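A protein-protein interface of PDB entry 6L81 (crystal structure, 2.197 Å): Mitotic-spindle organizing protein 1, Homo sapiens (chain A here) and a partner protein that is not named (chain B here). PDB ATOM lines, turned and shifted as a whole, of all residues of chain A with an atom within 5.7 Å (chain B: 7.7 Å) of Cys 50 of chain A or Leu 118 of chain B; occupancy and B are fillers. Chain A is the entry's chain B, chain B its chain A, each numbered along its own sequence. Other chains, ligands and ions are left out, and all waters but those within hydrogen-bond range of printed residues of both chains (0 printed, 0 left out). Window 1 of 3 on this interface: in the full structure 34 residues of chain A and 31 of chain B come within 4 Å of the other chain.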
ATOM      1  N   THR A  40     -16.381  12.446  -9.188  1.00  0.00           N
ATOM      2  CA  THR A  40     -17.769  12.902  -9.177  1.00  0.00           C
ATOM      3  C   THR A  40     -18.224  13.366  -7.801  1.00  0.00           C
ATOM      4  O   THR A  40     -19.257  14.038  -7.696  1.00  0.00           O
ATOM      5  CB  THR A  40     -18.714  11.788  -9.631  1.00  0.00           C
ATOM      6  OG1 THR A  40     -18.732  10.771  -8.625  1.00  0.00           O
ATOM      7  CG2 THR A  40     -18.280  11.183 -10.986  1.00  0.00           C
ATOM      8  N   LEU A  42     -19.348  11.295  -5.580  1.00  0.00           N
ATOM      9  CA  LEU A  42     -20.348  10.372  -5.062  1.00  0.00           C
ATOM     10  C   LEU A  42     -19.722   9.354  -4.118  1.00  0.00           C
ATOM     11  O   LEU A  42     -18.620   8.843  -4.352  1.00  0.00           O
ATOM     12  CB  LEU A  42     -21.079   9.631  -6.187  1.00  0.00           C
ATOM     13  CG  LEU A  42     -21.774  10.455  -7.271  1.00  0.00           C
ATOM     14  CD1 LEU A  42     -22.025   9.633  -8.481  1.00  0.00           C
ATOM     15  CD2 LEU A  42     -23.087  11.020  -6.747  1.00  0.00           C
ATOM     16  N   GLU A  45     -23.265   4.946  -1.305  1.00  0.00           N
ATOM     17  CA  GLU A  45     -24.701   4.948  -1.020  1.00  0.00           C
ATOM     18  C   GLU A  45     -25.467   5.773  -2.053  1.00  0.00           C
ATOM     19  O   GLU A  45     -26.470   5.313  -2.615  1.00  0.00           O
ATOM     20  CB  GLU A  45     -24.955   5.484   0.396  1.00  0.00           C
ATOM     21  CG  GLU A  45     -26.058   4.764   1.168  1.00  0.00           C
ATOM     22  CD  GLU A  45     -26.150   5.185   2.641  1.00  0.00           C
ATOM     23  OE1 GLU A  45     -25.170   5.758   3.177  1.00  0.00           O
ATOM     24  OE2 GLU A  45     -27.209   4.931   3.261  1.00  0.00           O
ATOM     25  N   THR A  46     -25.015   7.000  -2.315  1.00  0.00           N
ATOM     26  CA  THR A  46     -25.682   7.797  -3.334  1.00  0.00           C
ATOM     27  C   THR A  46     -25.430   7.240  -4.736  1.00  0.00           C
ATOM     28  O   THR A  46     -26.311   7.343  -5.605  1.00  0.00           O
ATOM     29  CB  THR A  46     -25.265   9.268  -3.213  1.00  0.00           C
ATOM     30  OG1 THR A  46     -23.855   9.393  -3.392  1.00  0.00           O
ATOM     31  CG2 THR A  46     -25.607   9.776  -1.825  1.00  0.00           C
ATOM     32  N   LEU A  47     -24.273   6.596  -4.963  1.00  0.00           N
ATOM     33  CA  LEU A  47     -24.022   6.006  -6.283  1.00  0.00           C
ATOM     34  C   LEU A  47     -25.026   4.899  -6.574  1.00  0.00           C
ATOM     35  O   LEU A  47     -25.567   4.814  -7.689  1.00  0.00           O
ATOM     36  CB  LEU A  47     -22.590   5.466  -6.389  1.00  0.00           C
ATOM     37  CG  LEU A  47     -22.315   4.599  -7.639  1.00  0.00           C
ATOM     38  CD1 LEU A  47     -22.550   5.386  -8.920  1.00  0.00           C
ATOM     39  CD2 LEU A  47     -20.887   4.041  -7.650  1.00  0.00           C
ATOM     40  N   SER A  48     -25.315   4.061  -5.564  1.00  0.00           N
ATOM     41  CA  SER A  48     -26.325   3.018  -5.722  1.00  0.00           C
ATOM     42  C   SER A  48     -27.686   3.610  -6.055  1.00  0.00           C
ATOM     43  O   SER A  48     -28.417   3.071  -6.895  1.00  0.00           O
ATOM     44  CB  SER A  48     -26.426   2.174  -4.448  1.00  0.00           C
ATOM     45  OG  SER A  48     -25.186   1.561  -4.158  1.00  0.00           O
ATOM     46  N   ILE A  49     -28.054   4.699  -5.379  1.00  0.00           N
ATOM     47  CA  ILE A  49     -29.299   5.392  -5.697  1.00  0.00           C
ATOM     48  C   ILE A  49     -29.311   5.779  -7.178  1.00  0.00           C
ATOM     49  O   ILE A  49     -30.261   5.485  -7.914  1.00  0.00           O
ATOM     50  CB  ILE A  49     -29.468   6.622  -4.783  1.00  0.00           C
ATOM     51  CG1 ILE A  49     -29.651   6.200  -3.320  1.00  0.00           C
ATOM     52  CG2 ILE A  49     -30.630   7.491  -5.247  1.00  0.00           C
ATOM     53  CD1 ILE A  49     -29.790   7.382  -2.366  1.00  0.00           C
ATOM     54  N   CYS A  50     -28.219   6.399  -7.643  1.00  0.00           N
ATOM     55  CA  CYS A  50     -28.141   6.829  -9.035  1.00  0.00           C
ATOM     56  C   CYS A  50     -28.272   5.658 -10.007  1.00  0.00           C
ATOM     57  O   CYS A  50     -28.972   5.766 -11.026  1.00  0.00           O
ATOM     58  CB  CYS A  50     -26.830   7.584  -9.266  1.00  0.00           C
ATOM     59  SG  CYS A  50     -26.845   9.185  -8.469  1.00  0.00           S
ATOM     60  N   VAL A  51     -27.623   4.530  -9.711  1.00  0.00           N
ATOM     61  CA  VAL A  51     -27.734   3.370 -10.601  1.00  0.00           C
ATOM     62  C   VAL A  51     -29.190   2.933 -10.748  1.00  0.00           C
ATOM     63  O   VAL A  51     -29.672   2.676 -11.859  1.00  0.00           O
ATOM     64  CB  VAL A  51     -26.853   2.211 -10.097  1.00  0.00           C
ATOM     65  CG1 VAL A  51     -27.179   0.914 -10.849  1.00  0.00           C
ATOM     66  CG2 VAL A  51     -25.391   2.560 -10.234  1.00  0.00           C
ATOM     67  N   ARG A  52     -29.903   2.809  -9.626  1.00  0.00           N
ATOM     68  CA  ARG A  52     -31.289   2.346  -9.695  1.00  0.00           C
ATOM     69  C   ARG A  52     -32.160   3.331 -10.469  1.00  0.00           C
ATOM     70  O   ARG A  52     -33.014   2.924 -11.261  1.00  0.00           O
ATOM     71  CB  ARG A  52     -31.850   2.136  -8.287  1.00  0.00           C
ATOM     72  CG  ARG A  52     -31.276   0.952  -7.517  1.00  0.00           C
ATOM     73  CD  ARG A  52     -31.905   0.865  -6.097  1.00  0.00           C
ATOM     74  NE  ARG A  52     -30.858   1.003  -5.088  1.00  0.00           N
ATOM     75  CZ  ARG A  52     -30.803   1.927  -4.136  1.00  0.00           C
ATOM     76  NH1 ARG A  52     -31.766   2.811  -3.987  1.00  0.00           N
ATOM     77  NH2 ARG A  52     -29.771   1.949  -3.311  1.00  0.00           N
ATOM     78  N   LEU A  53     -31.959   4.633 -10.248  1.00  0.00           N
ATOM     79  CA  LEU A  53     -32.733   5.628 -10.982  1.00  0.00           C
ATOM     80  C   LEU A  53     -32.463   5.533 -12.483  1.00  0.00           C
ATOM     81  O   LEU A  53     -33.398   5.592 -13.295  1.00  0.00           O
ATOM     82  CB  LEU A  53     -32.423   7.037 -10.449  1.00  0.00           C
ATOM     83  CG  LEU A  53     -32.908   7.343  -9.021  1.00  0.00           C
ATOM     84  CD1 LEU A  53     -32.439   8.708  -8.523  1.00  0.00           C
ATOM     85  CD2 LEU A  53     -34.427   7.212  -8.887  1.00  0.00           C
ATOM     86  N   CYS A  54     -31.196   5.357 -12.871  1.00  0.00           N
ATOM     87  CA  CYS A  54     -30.887   5.191 -14.291  1.00  0.00           C
ATOM     88  C   CYS A  54     -31.527   3.926 -14.857  1.00  0.00           C
ATOM     89  O   CYS A  54     -32.088   3.949 -15.960  1.00  0.00           O
ATOM     90  CB  CYS A  54     -29.374   5.170 -14.504  1.00  0.00           C
ATOM     91  SG  CYS A  54     -28.552   6.805 -14.276  1.00  0.00           S
ATOM     92  N   GLU A  55     -31.454   2.807 -14.121  1.00  0.00           N
ATOM     93  CA  GLU A  55     -32.098   1.573 -14.580  1.00  0.00           C
ATOM     94  C   GLU A  55     -33.604   1.736 -14.751  1.00  0.00           C
ATOM     95  O   GLU A  55     -34.196   1.094 -15.618  1.00  0.00           O
ATOM     96  CB  GLU A  55     -31.835   0.427 -13.604  1.00  0.00           C
ATOM     97  CG  GLU A  55     -30.413  -0.056 -13.599  1.00  0.00           C
ATOM     98  CD  GLU A  55     -30.130  -0.960 -12.413  1.00  0.00           C
ATOM     99  OE1 GLU A  55     -31.009  -1.080 -11.530  1.00  0.00           O
ATOM    100  OE2 GLU A  55     -29.033  -1.555 -12.374  1.00  0.00           O
ATOM    101  N   PRO A  60     -30.281  10.636 -17.455  1.00  0.00           N
ATOM    102  CA  PRO A  60     -29.074  10.906 -16.653  1.00  0.00           C
ATOM    103  C   PRO A  60     -28.698  12.365 -16.608  1.00  0.00           C
ATOM    104  O   PRO A  60     -28.109  12.816 -15.607  1.00  0.00           O
ATOM    105  CB  PRO A  60     -27.981  10.069 -17.347  1.00  0.00           C
ATOM    106  CG  PRO A  60     -28.490   9.886 -18.786  1.00  0.00           C
ATOM    107  CD  PRO A  60     -30.000   9.828 -18.664  1.00  0.00           C
ATOM    108  N   LEU A  63     -30.839  13.866 -14.063  1.00  0.00           N
ATOM    109  CA  LEU A  63     -30.365  13.492 -12.730  1.00  0.00           C
ATOM    110  C   LEU A  63     -29.104  14.265 -12.355  1.00  0.00           C
ATOM    111  O   LEU A  63     -28.933  14.672 -11.199  1.00  0.00           O
ATOM    112  CB  LEU A  63     -30.104  11.979 -12.683  1.00  0.00           C
ATOM    113  CG  LEU A  63     -29.609  11.404 -11.363  1.00  0.00           C
ATOM    114  CD1 LEU A  63     -30.592  11.760 -10.228  1.00  0.00           C
ATOM    115  CD2 LEU A  63     -29.487   9.902 -11.522  1.00  0.00           C
ATOM    116  N   SER A  64     -28.198  14.451 -13.322  1.00  0.00           N
ATOM    117  CA  SER A  64     -27.017  15.286 -13.105  1.00  0.00           C
ATOM    118  C   SER A  64     -27.415  16.713 -12.730  1.00  0.00           C
ATOM    119  O   SER A  64     -26.872  17.292 -11.785  1.00  0.00           O
ATOM    120  CB  SER A  64     -26.158  15.301 -14.378  1.00  0.00           C
ATOM    121  OG  SER A  64     -25.176  16.320 -14.329  1.00  0.00           O
ATOM    122  N   ILE A  67     -28.724  16.742  -9.169  1.00  0.00           N
ATOM    123  CA  ILE A  67     -27.720  16.538  -8.135  1.00  0.00           C
ATOM    124  C   ILE A  67     -26.873  17.794  -7.968  1.00  0.00           C
ATOM    125  O   ILE A  67     -26.517  18.177  -6.844  1.00  0.00           O
ATOM    126  CB  ILE A  67     -26.858  15.304  -8.455  1.00  0.00           C
ATOM    127  CG1 ILE A  67     -27.660  14.023  -8.185  1.00  0.00           C
ATOM    128  CG2 ILE A  67     -25.536  15.331  -7.658  1.00  0.00           C
ATOM    129  CD1 ILE A  67     -27.085  12.791  -8.857  1.00  0.00           C
ATOM    130  N   ASP B  23     -36.245   6.208  -3.433  1.00  0.00           N
ATOM    131  CA  ASP B  23     -34.916   6.556  -3.917  1.00  0.00           C
ATOM    132  C   ASP B  23     -34.762   8.064  -4.090  1.00  0.00           C
ATOM    133  O   ASP B  23     -33.741   8.635  -3.685  1.00  0.00           O
ATOM    134  CB  ASP B  23     -34.635   5.816  -5.220  1.00  0.00           C
ATOM    135  CG  ASP B  23     -34.237   4.357  -4.993  1.00  0.00           C
ATOM    136  OD1 ASP B  23     -33.882   4.003  -3.847  1.00  0.00           O
ATOM    137  OD2 ASP B  23     -34.270   3.569  -5.965  1.00  0.00           O
ATOM    138  N   LEU B  27     -32.133  10.373  -2.203  1.00  0.00           N
ATOM    139  CA  LEU B  27     -31.237  11.236  -2.967  1.00  0.00           C
ATOM    140  C   LEU B  27     -31.241  12.657  -2.413  1.00  0.00           C
ATOM    141  O   LEU B  27     -30.183  13.281  -2.280  1.00  0.00           O
ATOM    142  CB  LEU B  27     -31.633  11.229  -4.449  1.00  0.00           C
ATOM    143  CG  LEU B  27     -30.713  12.060  -5.347  1.00  0.00           C
ATOM    144  CD1 LEU B  27     -29.362  11.350  -5.527  1.00  0.00           C
ATOM    145  CD2 LEU B  27     -31.366  12.382  -6.700  1.00  0.00           C
ATOM    146  N   VAL B  31     -27.865  13.990  -0.849  1.00  0.00           N
ATOM    147  CA  VAL B  31     -27.108  15.006  -1.570  1.00  0.00           C
ATOM    148  C   VAL B  31     -27.297  16.377  -0.929  1.00  0.00           C
ATOM    149  O   VAL B  31     -26.334  17.127  -0.733  1.00  0.00           O
ATOM    150  CB  VAL B  31     -27.517  15.015  -3.048  1.00  0.00           C
ATOM    151  CG1 VAL B  31     -26.682  16.008  -3.798  1.00  0.00           C
ATOM    152  CG2 VAL B  31     -27.363  13.632  -3.630  1.00  0.00           C
ATOM    153  N   VAL B  61     -29.816   8.995 -24.420  1.00  0.00           N
ATOM    154  CA  VAL B  61     -28.373   8.835 -24.321  1.00  0.00           C
ATOM    155  C   VAL B  61     -27.859   8.157 -25.583  1.00  0.00           C
ATOM    156  O   VAL B  61     -28.446   7.183 -26.072  1.00  0.00           O
ATOM    157  CB  VAL B  61     -27.989   8.068 -23.048  1.00  0.00           C
ATOM    158  CG1 VAL B  61     -28.756   6.774 -22.951  1.00  0.00           C
ATOM    159  CG2 VAL B  61     -26.472   7.818 -23.021  1.00  0.00           C
ATOM    160  N   ILE B  66     -20.951   8.121 -25.890  1.00  0.00           N
ATOM    161  CA  ILE B  66     -20.378   7.776 -24.596  1.00  0.00           C
ATOM    162  C   ILE B  66     -19.093   6.978 -24.794  1.00  0.00           C
ATOM    163  O   ILE B  66     -18.075   7.222 -24.130  1.00  0.00           O
ATOM    164  CB  ILE B  66     -21.394   6.990 -23.740  1.00  0.00           C
ATOM    165  CG1 ILE B  66     -22.685   7.802 -23.527  1.00  0.00           C
ATOM    166  CG2 ILE B  66     -20.767   6.621 -22.401  1.00  0.00           C
ATOM    167  CD1 ILE B  66     -22.438   9.230 -23.087  1.00  0.00           C
ATOM    168  N   HIS B 112     -26.151   0.689 -19.003  1.00  0.00           N
ATOM    169  CA  HIS B 112     -24.706   0.892 -18.891  1.00  0.00           C
ATOM    170  C   HIS B 112     -24.338   2.318 -19.266  1.00  0.00           C
ATOM    171  O   HIS B 112     -23.601   2.993 -18.540  1.00  0.00           O
ATOM    172  CB  HIS B 112     -23.925  -0.076 -19.788  1.00  0.00           C
ATOM    173  CG  HIS B 112     -24.047  -1.521 -19.411  1.00  0.00           C
ATOM    174  ND1 HIS B 112     -23.146  -2.152 -18.578  1.00  0.00           N
ATOM    175  CD2 HIS B 112     -24.932  -2.471 -19.793  1.00  0.00           C
ATOM    176  CE1 HIS B 112     -23.488  -3.419 -18.438  1.00  0.00           C
ATOM    177  NE2 HIS B 112     -24.571  -3.639 -19.163  1.00  0.00           N
ATOM    178  N   TYR B 113     -24.836   2.784 -20.417  1.00  0.00           N
ATOM    179  CA  TYR B 113     -24.430   4.073 -20.951  1.00  0.00           C
ATOM    180  C   TYR B 113     -25.122   5.217 -20.243  1.00  0.00           C
ATOM    181  O   TYR B 113     -24.529   6.288 -20.085  1.00  0.00           O
ATOM    182  CB  TYR B 113     -24.685   4.107 -22.457  1.00  0.00           C
ATOM    183  CG  TYR B 113     -23.845   3.066 -23.130  1.00  0.00           C
ATOM    184  CD1 TYR B 113     -22.482   3.269 -23.322  1.00  0.00           C
ATOM    185  CD2 TYR B 113     -24.390   1.854 -23.517  1.00  0.00           C
ATOM    186  CE1 TYR B 113     -21.698   2.297 -23.913  1.00  0.00           C
ATOM    187  CE2 TYR B 113     -23.614   0.879 -24.104  1.00  0.00           C
ATOM    188  CZ  TYR B 113     -22.277   1.101 -24.297  1.00  0.00           C
ATOM    189  OH  TYR B 113     -21.526   0.117 -24.889  1.00  0.00           O
ATOM    190  N   SER B 114     -26.346   4.996 -19.769  1.00  0.00           N
ATOM    191  CA  SER B 114     -27.004   6.013 -18.962  1.00  0.00           C
ATOM    192  C   SER B 114     -26.243   6.260 -17.660  1.00  0.00           C
ATOM    193  O   SER B 114     -26.022   7.411 -17.267  1.00  0.00           O
ATOM    194  CB  SER B 114     -28.443   5.593 -18.682  1.00  0.00           C
ATOM    195  OG  SER B 114     -29.021   6.527 -17.807  1.00  0.00           O
ATOM    196  N   ILE B 115     -25.849   5.195 -16.964  1.00  0.00           N
ATOM    197  CA  ILE B 115     -25.031   5.355 -15.761  1.00  0.00           C
ATOM    198  C   ILE B 115     -23.739   6.092 -16.096  1.00  0.00           C
ATOM    199  O   ILE B 115     -23.346   7.043 -15.408  1.00  0.00           O
ATOM    200  CB  ILE B 115     -24.736   3.979 -15.125  1.00  0.00           C
ATOM    201  CG1 ILE B 115     -26.018   3.376 -14.514  1.00  0.00           C
ATOM    202  CG2 ILE B 115     -23.596   4.093 -14.102  1.00  0.00           C
ATOM    203  CD1 ILE B 115     -25.989   1.851 -14.370  1.00  0.00           C
ATOM    204  N   LEU B 116     -23.058   5.660 -17.162  1.00  0.00           N
ATOM    205  CA  LEU B 116     -21.777   6.275 -17.501  1.00  0.00           C
ATOM    206  C   LEU B 116     -21.954   7.745 -17.872  1.00  0.00           C
ATOM    207  O   LEU B 116     -21.148   8.593 -17.482  1.00  0.00           O
ATOM    208  CB  LEU B 116     -21.126   5.502 -18.646  1.00  0.00           C
ATOM    209  CG  LEU B 116     -19.983   4.507 -18.395  1.00  0.00           C
ATOM    210  CD1 LEU B 116     -19.679   4.245 -16.947  1.00  0.00           C
ATOM    211  CD2 LEU B 116     -20.222   3.215 -19.140  1.00  0.00           C
ATOM    212  N   SER B 117     -23.019   8.062 -18.616  1.00  0.00           N
ATOM    213  CA  SER B 117     -23.316   9.451 -18.942  1.00  0.00           C
ATOM    214  C   SER B 117     -23.505  10.294 -17.680  1.00  0.00           C
ATOM    215  O   SER B 117     -23.003  11.425 -17.593  1.00  0.00           O
ATOM    216  CB  SER B 117     -24.560   9.515 -19.828  1.00  0.00           C
ATOM    217  OG  SER B 117     -25.006  10.840 -19.974  1.00  0.00           O
ATOM    218  N   LEU B 118     -24.231   9.772 -16.687  1.00  0.00           N
ATOM    219  CA  LEU B 118     -24.377  10.530 -15.449  1.00  0.00           C
ATOM    220  C   LEU B 118     -23.013  10.798 -14.811  1.00  0.00           C
ATOM    221  O   LEU B 118     -22.717  11.923 -14.399  1.00  0.00           O
ATOM    222  CB  LEU B 118     -25.279   9.788 -14.464  1.00  0.00           C
ATOM    223  CG  LEU B 118     -25.148  10.323 -13.033  1.00  0.00           C
ATOM    224  CD1 LEU B 118     -25.902  11.656 -12.837  1.00  0.00           C
ATOM    225  CD2 LEU B 118     -25.572   9.284 -11.991  1.00  0.00           C
ATOM    226  N   LEU B 119     -22.169   9.762 -14.705  1.00  0.00           N
ATOM    227  CA  LEU B 119     -20.867   9.971 -14.074  1.00  0.00           C
ATOM    228  C   LEU B 119     -20.028  10.963 -14.879  1.00  0.00           C
ATOM    229  O   LEU B 119     -19.355  11.831 -14.307  1.00  0.00           O
ATOM    230  CB  LEU B 119     -20.134   8.636 -13.915  1.00  0.00           C
ATOM    231  CG  LEU B 119     -20.901   7.591 -13.093  1.00  0.00           C
ATOM    232  CD1 LEU B 119     -20.088   6.314 -12.935  1.00  0.00           C
ATOM    233  CD2 LEU B 119     -21.279   8.161 -11.724  1.00  0.00           C
ATOM    234  N   LEU B 120     -20.099  10.877 -16.208  1.00  0.00           N
ATOM    235  CA  LEU B 120     -19.383  11.840 -17.039  1.00  0.00           C
ATOM    236  C   LEU B 120     -19.901  13.252 -16.799  1.00  0.00           C
ATOM    237  O   LEU B 120     -19.118  14.198 -16.710  1.00  0.00           O
ATOM    238  CB  LEU B 120     -19.502  11.452 -18.513  1.00  0.00           C
ATOM    239  CG  LEU B 120     -18.689  10.210 -18.902  1.00  0.00           C
ATOM    240  CD1 LEU B 120     -19.046   9.689 -20.288  1.00  0.00           C
ATOM    241  CD2 LEU B 120     -17.142  10.461 -18.795  1.00  0.00           C
ATOM    242  N   CYS B 121     -21.215  13.408 -16.651  1.00  0.00           N
ATOM    243  CA  CYS B 121     -21.769  14.726 -16.388  1.00  0.00           C
ATOM    244  C   CYS B 121     -21.353  15.267 -15.020  1.00  0.00           C
ATOM    245  O   CYS B 121     -21.188  16.481 -14.862  1.00  0.00           O
ATOM    246  CB  CYS B 121     -23.294  14.673 -16.506  1.00  0.00           C
ATOM    247  SG  CYS B 121     -23.838  15.057 -18.171  1.00  0.00           S
ATOM    248  N   LEU B 122     -21.182  14.392 -14.031  1.00  0.00           N
ATOM    249  CA  LEU B 122     -20.740  14.817 -12.707  1.00  0.00           C
ATOM    250  C   LEU B 122     -19.223  15.005 -12.595  1.00  0.00           C
ATOM    251  O   LEU B 122     -18.751  15.484 -11.564  1.00  0.00           O
ATOM    252  CB  LEU B 122     -21.215  13.801 -11.666  1.00  0.00           C
ATOM    253  CG  LEU B 122     -22.732  13.722 -11.465  1.00  0.00           C
ATOM    254  CD1 LEU B 122     -23.069  12.656 -10.421  1.00  0.00           C
ATOM    255  CD2 LEU B 122     -23.277  15.073 -11.045  1.00  0.00           C
ATOM    256  N   SER B 123     -18.447  14.632 -13.609  1.00  0.00           N
ATOM    257  CA  SER B 123     -17.006  14.853 -13.579  1.00  0.00           C
ATOM    258  C   SER B 123     -16.698  16.365 -13.555  1.00  0.00           C
ATOM    259  O   SER B 123     -15.898  16.805 -12.730  1.00  0.00           O
ATOM    260  CB  SER B 123     -16.325  14.179 -14.790  1.00  0.00           C
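Of the printed residues of chain B, Val 51 of chain A touches Ile 115. Glu 55 of chain A touches none of the printed residues of chain B. Of the printed residues of chain A, Leu 27 of chain B touches Ile 49 and Leu 63. Val 61 of chain B touches none of the printed residues of chain A. The nearest printed residue of chain A that does not touch Asp 23 of chain B is Ser 48 of chain A (5.9 Å).
Hydrophobic or aromatic side chains of chain B within 4 Å of the printed part of chain A: Leu 27, Val 31, Ile 115, Leu 118, Leu 119 and Leu 122. Along chain B the printed residues that touch a printed residue of chain A span positions 23 to 122. Printed residues of chain A that touch a printed residue of chain B: Thr 40, Leu 42, Ile 49, Cys 50, Val 51, Arg 52, Leu 53, Cys 54, Pro 60, Leu 63, Ser 64 and Ile 67. Among the printed residues, 21 pairs touch across the chains. Among the printed residues, Asp or Glu carboxylates within 4 Å of a Lys or Arg side-chain nitrogen of the other chain: Arg 52 of chain A with Asp 23 of chain B.
SG of Cys 121 of chain B lies close to O of Ser 117 of chain B, at 3.8 Å. The side-chain hydroxyl of Thr 40 of chain A is in hydrogen-bond range of the backbone NH of Leu 42 of chain A (3.2 Å). SG of Cys 50 of chain A sits at hydrogen-bond distance from O of Thr 46 of chain A (3.4 Å). The backbone carbonyl oxygen of Cys 50 of chain A lies within hydrogen-bond range of the side-chain sulfur of Cys 54 of chain A, at 3.4 Å.
The side-chain carboxylate of Asp 23 of chain B is in salt-bridge range of the guanidinium group of Arg 52 of chain A. The side-chain sulfur (SG) of Cys 54 of chain A is in hydrogen-bond range of the side-chain hydroxyl (OG) of Ser 114 of chain B (3.6 Å).
Leu 119 of chain B touches Thr 40 of chain A (O to CG2, 3.6 Å). Thr 40 of chain A touches Leu 122 of chain B. Ile 49 of chain A touches Asp 23 of chain B (CG2 to O, 3.7 Å). Leu 27 of chain B touches Ile 49 of chain A (N to CD1, 3.8 Å). Leu 53 of chain A touches Asp 23 of chain B. Cys 54 of chain A touches Ile 115 of chain B (CB to CG1, 3.8 Å). Leu 118 of chain B touches Leu 63 of chain A (CD2 to CD2, 3.99 Å). Ser 64 of chain A touches Leu 118 of chain B. Ser 64 of chain A touches Leu 122 of chain B. O of Ile 67 of chain A touches CG1 of Val 31 of chain B (3.7 Å).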
